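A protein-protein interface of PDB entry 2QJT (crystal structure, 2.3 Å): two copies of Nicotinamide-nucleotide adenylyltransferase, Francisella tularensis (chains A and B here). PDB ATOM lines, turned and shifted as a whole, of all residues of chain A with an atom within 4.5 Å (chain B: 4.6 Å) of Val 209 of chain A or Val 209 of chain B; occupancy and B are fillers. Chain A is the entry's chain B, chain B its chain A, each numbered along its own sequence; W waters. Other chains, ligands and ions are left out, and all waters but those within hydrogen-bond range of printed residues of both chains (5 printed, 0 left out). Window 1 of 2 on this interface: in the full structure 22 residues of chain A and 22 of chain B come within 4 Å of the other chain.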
ATOM      1  N   ASN A 207      16.247 -17.145 -26.253  1.00  0.00           N
ATOM      2  CA  ASN A 207      15.807 -18.012 -27.337  1.00  0.00           C
ATOM      3  C   ASN A 207      15.637 -17.100 -28.546  1.00  0.00           C
ATOM      4  O   ASN A 207      14.799 -16.190 -28.542  1.00  0.00           O
ATOM      5  CB  ASN A 207      14.464 -18.721 -27.046  1.00  0.00           C
ATOM      6  CG  ASN A 207      14.493 -19.595 -25.813  1.00  0.00           C
ATOM      7  OD1 ASN A 207      15.150 -20.646 -25.763  1.00  0.00           O
ATOM      8  ND2 ASN A 207      13.742 -19.193 -24.831  1.00  0.00           N
ATOM      9  N   PHE A 208      16.442 -17.344 -29.562  1.00  0.00           N
ATOM     10  CA  PHE A 208      16.371 -16.613 -30.815  1.00  0.00           C
ATOM     11  C   PHE A 208      15.290 -17.179 -31.723  1.00  0.00           C
ATOM     12  O   PHE A 208      15.100 -18.408 -31.815  1.00  0.00           O
ATOM     13  CB  PHE A 208      17.720 -16.665 -31.540  1.00  0.00           C
ATOM     14  CG  PHE A 208      18.871 -16.120 -30.728  1.00  0.00           C
ATOM     15  CD1 PHE A 208      19.853 -16.982 -30.224  1.00  0.00           C
ATOM     16  CD2 PHE A 208      18.965 -14.762 -30.457  1.00  0.00           C
ATOM     17  CE1 PHE A 208      20.916 -16.502 -29.489  1.00  0.00           C
ATOM     18  CE2 PHE A 208      20.030 -14.256 -29.721  1.00  0.00           C
ATOM     19  CZ  PHE A 208      21.011 -15.120 -29.236  1.00  0.00           C
ATOM     20  N   VAL A 209      14.608 -16.270 -32.413  1.00  0.00           N
ATOM     21  CA  VAL A 209      13.535 -16.617 -33.352  1.00  0.00           C
ATOM     22  C   VAL A 209      13.939 -16.210 -34.771  1.00  0.00           C
ATOM     23  O   VAL A 209      14.279 -15.050 -35.044  1.00  0.00           O
ATOM     24  CB  VAL A 209      12.143 -16.001 -32.941  1.00  0.00           C
ATOM     25  CG1 VAL A 209      11.008 -16.601 -33.777  1.00  0.00           C
ATOM     26  CG2 VAL A 209      11.853 -16.218 -31.418  1.00  0.00           C
ATOM     27  N   THR A 210      13.909 -17.192 -35.658  1.00  0.00           N
ATOM     28  CA  THR A 210      14.167 -17.021 -37.059  1.00  0.00           C
ATOM     29  C   THR A 210      12.999 -17.546 -37.906  1.00  0.00           C
ATOM     30  O   THR A 210      12.091 -18.228 -37.408  1.00  0.00           O
ATOM     31  CB  THR A 210      15.495 -17.709 -37.508  1.00  0.00           C
ATOM     32  OG1 THR A 210      15.353 -19.126 -37.443  1.00  0.00           O
ATOM     33  CG2 THR A 210      16.671 -17.245 -36.662  1.00  0.00           C
ATOM     34  N   PHE A 241      16.338 -13.461 -39.160  1.00  0.00           N
ATOM     35  CA  PHE A 241      15.790 -13.130 -37.867  1.00  0.00           C
ATOM     36  C   PHE A 241      14.442 -12.469 -38.013  1.00  0.00           C
ATOM     37  O   PHE A 241      14.196 -11.674 -38.931  1.00  0.00           O
ATOM     38  CB  PHE A 241      16.796 -12.278 -37.060  1.00  0.00           C
ATOM     39  CG  PHE A 241      17.948 -13.091 -36.483  1.00  0.00           C
ATOM     40  CD1 PHE A 241      19.144 -13.223 -37.179  1.00  0.00           C
ATOM     41  CD2 PHE A 241      17.811 -13.766 -35.253  1.00  0.00           C
ATOM     42  CE1 PHE A 241      20.213 -14.016 -36.650  1.00  0.00           C
ATOM     43  CE2 PHE A 241      18.871 -14.557 -34.718  1.00  0.00           C
ATOM     44  CZ  PHE A 241      20.062 -14.680 -35.426  1.00  0.00           C
ATOM     45  N   LEU A 242      13.551 -12.835 -37.115  1.00  0.00           N
ATOM     46  CA  LEU A 242      12.271 -12.178 -36.953  1.00  0.00           C
ATOM     47  C   LEU A 242      12.484 -10.862 -36.212  1.00  0.00           C
ATOM     48  O   LEU A 242      13.170 -10.816 -35.167  1.00  0.00           O
ATOM     49  CB  LEU A 242      11.343 -13.099 -36.148  1.00  0.00           C
ATOM     50  CG  LEU A 242      10.058 -12.490 -35.601  1.00  0.00           C
ATOM     51  CD1 LEU A 242       9.104 -12.199 -36.757  1.00  0.00           C
ATOM     52  CD2 LEU A 242       9.432 -13.425 -34.578  1.00  0.00           C
ATOM     53  N   ILE A 291      15.030 -21.032 -32.581  1.00  0.00           N
ATOM     54  CA  ILE A 291      13.803 -21.683 -33.052  1.00  0.00           C
ATOM     55  C   ILE A 291      13.460 -21.123 -34.429  1.00  0.00           C
ATOM     56  O   ILE A 291      13.489 -19.913 -34.640  1.00  0.00           O
ATOM     57  CB  ILE A 291      12.628 -21.401 -32.120  1.00  0.00           C
ATOM     58  CG1 ILE A 291      12.916 -21.960 -30.726  1.00  0.00           C
ATOM     59  CG2 ILE A 291      11.294 -22.043 -32.646  1.00  0.00           C
ATOM     60  CD1 ILE A 291      12.065 -21.297 -29.596  1.00  0.00           C
ATOM     61  N   HIS A 293      10.583 -20.885 -37.648  1.00  0.00           N
ATOM     62  CA  HIS A 293       9.251 -21.076 -38.215  1.00  0.00           C
ATOM     63  C   HIS A 293       9.380 -21.023 -39.741  1.00  0.00           C
ATOM     64  O   HIS A 293       9.830 -20.032 -40.281  1.00  0.00           O
ATOM     65  CB  HIS A 293       8.279 -19.974 -37.766  1.00  0.00           C
ATOM     66  CG  HIS A 293       8.201 -19.766 -36.288  1.00  0.00           C
ATOM     67  ND1 HIS A 293       7.073 -20.073 -35.554  1.00  0.00           N
ATOM     68  CD2 HIS A 293       9.092 -19.234 -35.406  1.00  0.00           C
ATOM     69  CE1 HIS A 293       7.286 -19.775 -34.282  1.00  0.00           C
ATOM     70  NE2 HIS A 293       8.496 -19.251 -34.166  1.00  0.00           N
ATOM     71  N   ASN B 207      13.043 -10.902 -28.804  1.00  0.00           N
ATOM     72  CA  ASN B 207      11.755 -11.589 -28.881  1.00  0.00           C
ATOM     73  C   ASN B 207      11.712 -12.549 -27.678  1.00  0.00           C
ATOM     74  O   ASN B 207      12.640 -13.324 -27.466  1.00  0.00           O
ATOM     75  CB  ASN B 207      11.620 -12.387 -30.176  1.00  0.00           C
ATOM     76  CG  ASN B 207      11.510 -11.519 -31.422  1.00  0.00           C
ATOM     77  OD1 ASN B 207      10.671 -10.635 -31.527  1.00  0.00           O
ATOM     78  ND2 ASN B 207      12.339 -11.811 -32.396  1.00  0.00           N
ATOM     79  N   PHE B 208      10.667 -12.471 -26.861  1.00  0.00           N
ATOM     80  CA  PHE B 208      10.515 -13.452 -25.809  1.00  0.00           C
ATOM     81  C   PHE B 208       9.701 -14.623 -26.345  1.00  0.00           C
ATOM     82  O   PHE B 208       8.790 -14.456 -27.182  1.00  0.00           O
ATOM     83  CB  PHE B 208       9.941 -12.819 -24.563  1.00  0.00           C
ATOM     84  CG  PHE B 208      10.816 -11.696 -23.999  1.00  0.00           C
ATOM     85  CD1 PHE B 208      10.346 -10.362 -23.965  1.00  0.00           C
ATOM     86  CD2 PHE B 208      12.093 -11.959 -23.526  1.00  0.00           C
ATOM     87  CE1 PHE B 208      11.124  -9.351 -23.479  1.00  0.00           C
ATOM     88  CE2 PHE B 208      12.882 -10.933 -23.021  1.00  0.00           C
ATOM     89  CZ  PHE B 208      12.402  -9.623 -23.008  1.00  0.00           C
ATOM     90  N   VAL B 209      10.086 -15.815 -25.920  1.00  0.00           N
ATOM     91  CA  VAL B 209       9.355 -17.032 -26.260  1.00  0.00           C
ATOM     92  C   VAL B 209       8.739 -17.665 -25.014  1.00  0.00           C
ATOM     93  O   VAL B 209       9.440 -18.045 -24.095  1.00  0.00           O
ATOM     94  CB  VAL B 209      10.196 -18.046 -27.065  1.00  0.00           C
ATOM     95  CG1 VAL B 209       9.295 -19.233 -27.542  1.00  0.00           C
ATOM     96  CG2 VAL B 209      10.796 -17.382 -28.263  1.00  0.00           C
ATOM     97  N   THR B 210       7.412 -17.743 -24.991  1.00  0.00           N
ATOM     98  CA  THR B 210       6.687 -18.359 -23.879  1.00  0.00           C
ATOM     99  C   THR B 210       5.852 -19.541 -24.381  1.00  0.00           C
ATOM    100  O   THR B 210       5.771 -19.795 -25.573  1.00  0.00           O
ATOM    101  CB  THR B 210       5.800 -17.323 -23.103  1.00  0.00           C
ATOM    102  OG1 THR B 210       4.777 -16.829 -23.976  1.00  0.00           O
ATOM    103  CG2 THR B 210       6.631 -16.116 -22.598  1.00  0.00           C
ATOM    104  N   PHE B 241       7.991 -18.922 -19.439  1.00  0.00           N
ATOM    105  CA  PHE B 241       9.063 -18.783 -20.413  1.00  0.00           C
ATOM    106  C   PHE B 241       9.581 -20.127 -20.826  1.00  0.00           C
ATOM    107  O   PHE B 241       9.717 -21.016 -20.007  1.00  0.00           O
ATOM    108  CB  PHE B 241      10.205 -17.902 -19.885  1.00  0.00           C
ATOM    109  CG  PHE B 241       9.823 -16.484 -19.750  1.00  0.00           C
ATOM    110  CD1 PHE B 241       9.308 -15.998 -18.560  1.00  0.00           C
ATOM    111  CD2 PHE B 241       9.935 -15.621 -20.840  1.00  0.00           C
ATOM    112  CE1 PHE B 241       8.876 -14.642 -18.467  1.00  0.00           C
ATOM    113  CE2 PHE B 241       9.537 -14.298 -20.764  1.00  0.00           C
ATOM    114  CZ  PHE B 241       9.000 -13.809 -19.579  1.00  0.00           C
ATOM    115  N   LEU B 242       9.845 -20.260 -22.124  1.00  0.00           N
ATOM    116  CA  LEU B 242      10.610 -21.353 -22.658  1.00  0.00           C
ATOM    117  C   LEU B 242      12.078 -21.263 -22.175  1.00  0.00           C
ATOM    118  O   LEU B 242      12.689 -20.190 -22.217  1.00  0.00           O
ATOM    119  CB  LEU B 242      10.565 -21.290 -24.178  1.00  0.00           C
ATOM    120  CG  LEU B 242      11.393 -22.334 -24.932  1.00  0.00           C
ATOM    121  CD1 LEU B 242      10.853 -23.765 -24.710  1.00  0.00           C
ATOM    122  CD2 LEU B 242      11.438 -21.976 -26.391  1.00  0.00           C
ATOM    123  N   ILE B 291       6.152 -14.031 -28.100  1.00  0.00           N
ATOM    124  CA  ILE B 291       5.506 -15.027 -28.928  1.00  0.00           C
ATOM    125  C   ILE B 291       5.183 -16.197 -28.038  1.00  0.00           C
ATOM    126  O   ILE B 291       6.064 -16.726 -27.316  1.00  0.00           O
ATOM    127  CB  ILE B 291       6.437 -15.511 -30.038  1.00  0.00           C
ATOM    128  CG1 ILE B 291       6.869 -14.325 -30.901  1.00  0.00           C
ATOM    129  CG2 ILE B 291       5.733 -16.591 -30.935  1.00  0.00           C
ATOM    130  CD1 ILE B 291       8.076 -14.575 -31.691  1.00  0.00           C
ATOM    131  N   HIS B 293       3.603 -20.175 -27.618  1.00  0.00           N
ATOM    132  CA  HIS B 293       3.203 -21.431 -28.228  1.00  0.00           C
ATOM    133  C   HIS B 293       2.236 -22.093 -27.262  1.00  0.00           C
ATOM    134  O   HIS B 293       2.596 -22.349 -26.128  1.00  0.00           O
ATOM    135  CB  HIS B 293       4.399 -22.340 -28.477  1.00  0.00           C
ATOM    136  CG  HIS B 293       5.462 -21.730 -29.328  1.00  0.00           C
ATOM    137  ND1 HIS B 293       5.798 -22.223 -30.566  1.00  0.00           N
ATOM    138  CD2 HIS B 293       6.300 -20.695 -29.101  1.00  0.00           C
ATOM    139  CE1 HIS B 293       6.794 -21.509 -31.072  1.00  0.00           C
ATOM    140  NE2 HIS B 293       7.110 -20.571 -30.201  1.00  0.00           N
HETATM  141  O   HOH W   1      14.059 -14.788 -25.771  1.00  0.00           O
HETATM  142  O   HOH W   2      15.497 -13.103 -28.902  1.00  0.00           O
HETATM  143  O   HOH W   3      12.711 -16.623 -24.384  1.00  0.00           O
HETATM  144  O   HOH W   4      15.012 -12.877 -33.215  1.00  0.00           O
HETATM  145  O   HOH W   5       9.014 -18.884 -31.365  1.00  0.00           O
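Of the 8 printed residues of chain B, 5 touch a printed residue of chain A. Hydrophobic or aromatic side chains of chain B within 4 Å of the printed part of chain A: Val 209, Leu 242, Ile 291 and His 293. Among the printed residues, 7 pairs touch across the chains. Among the printed residues, no Asp or Glu carboxylate lies within 4 Å of a Lys or Arg side-chain nitrogen of the other chain.
The backbone carbonyl oxygen (O) of Val 209 of chain A sits at hydrogen-bond distance from the backbone NH (N) of Leu 242 of chain A (3.1 Å). The backbone NH (N) of Thr 210 of chain A lies within hydrogen-bond range of the backbone carbonyl oxygen (O) of Ile 291 of chain A (2.9 Å). N of His 293 of chain A lies within hydrogen-bond range of O of Thr 210 of chain A (3.1 Å). O of Phe 208 of chain B lies within hydrogen-bond range of N of Ile 291 of chain B, at 2.8 Å. The backbone NH of Leu 242 of chain B is in hydrogen-bond range of the backbone carbonyl oxygen of Val 209 of chain B (3.0 Å). The backbone carbonyl oxygen (O) of Thr 210 of chain B is in hydrogen-bond range of the backbone NH (N) of His 293 of chain B, 3.0 Å away.
Among the printed residues, pairs that only touch across the chains: Ile 291 of chain A with Leu 242 of chain B (3.3 Å), Leu 242 of chain A with Ile 291 of chain B (3.4 Å), Val 209 of chain A with Val 209 of chain B (3.5 Å), His 293 of chain A with His 293 of chain B (3.7 Å) and Asn 207 of chain A with Asn 207 of chain B (3.7 Å).
Val 209 of chain A touches just one residue of chain B: Val 209. Of the printed residues of chain A, Val 209 of chain B touches Val 209 (3.5 Å). Of the printed residues of chain A, Ile 291 of chain B touches Leu 242 (3.4 Å). Of the printed residues of chain B, Asn 207 of chain A touches Asn 207 and Leu 242. Of the printed residues of chain B, His 293 of chain A touches His 293 (3.7 Å). Thr 210 of chain B touches none of the printed residues of chain A. The nearest residue of chain B that does not touch Val 209 of chain A is Asn 207 of chain B (4.03 Å).
Asn 207 of chain B touches its own counterpart, Asn 207 of chain A. Val 209 of chain A touches its own counterpart, Val 209 of chain B. Leu 242 of chain A touches Ile 291 of chain B, and with the chains exchanged Ile 291 of chain A touches Leu 242 of chain B. His 293 of chain A touches its own counterpart, His 293 of chain B. 8 positions are printed for both chains. Of the 7 pairs that touch across the chains among the printed residues, 7 have their exchanged pair printed and touching as well.
Water W1 bridges O of Asn 207 of chain B (2.7 Å) and O of Asn 207 of chain A (3.2 Å). Water W5 lies within hydrogen-bond range of a ring nitrogen (NE2) of His 293 of chain B (2.8 Å) and a ring nitrogen (NE2) of His 293 of chain A (2.9 Å). Water W3 lies within hydrogen-bond range of ND2 of Asn 207 of chain A and N of Val 209 of chain B. Water W4 lies within hydrogen-bond range of the backbone carbonyl oxygen (O) of Val 209 of chain A (2.9 Å), the side-chain amide nitrogen (ND2) of Asn 207 of chain B (3.0 Å) and the backbone carbonyl oxygen (O) of Leu 242 of chain A (3.4 Å). Water W2 bridges the backbone carbonyl oxygen of Asn 207 of chain A and the backbone carbonyl oxygen of Asn 207 of chain B.
O of Leu 242 of chain B lies within hydrogen-bond range of ND2 of Asn 207 of chain A (3.0 Å). The backbone carbonyl oxygen (O) of Leu 242 of chain A sits at hydrogen-bond distance from the side-chain amide nitrogen (ND2) of Asn 207 of chain B.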
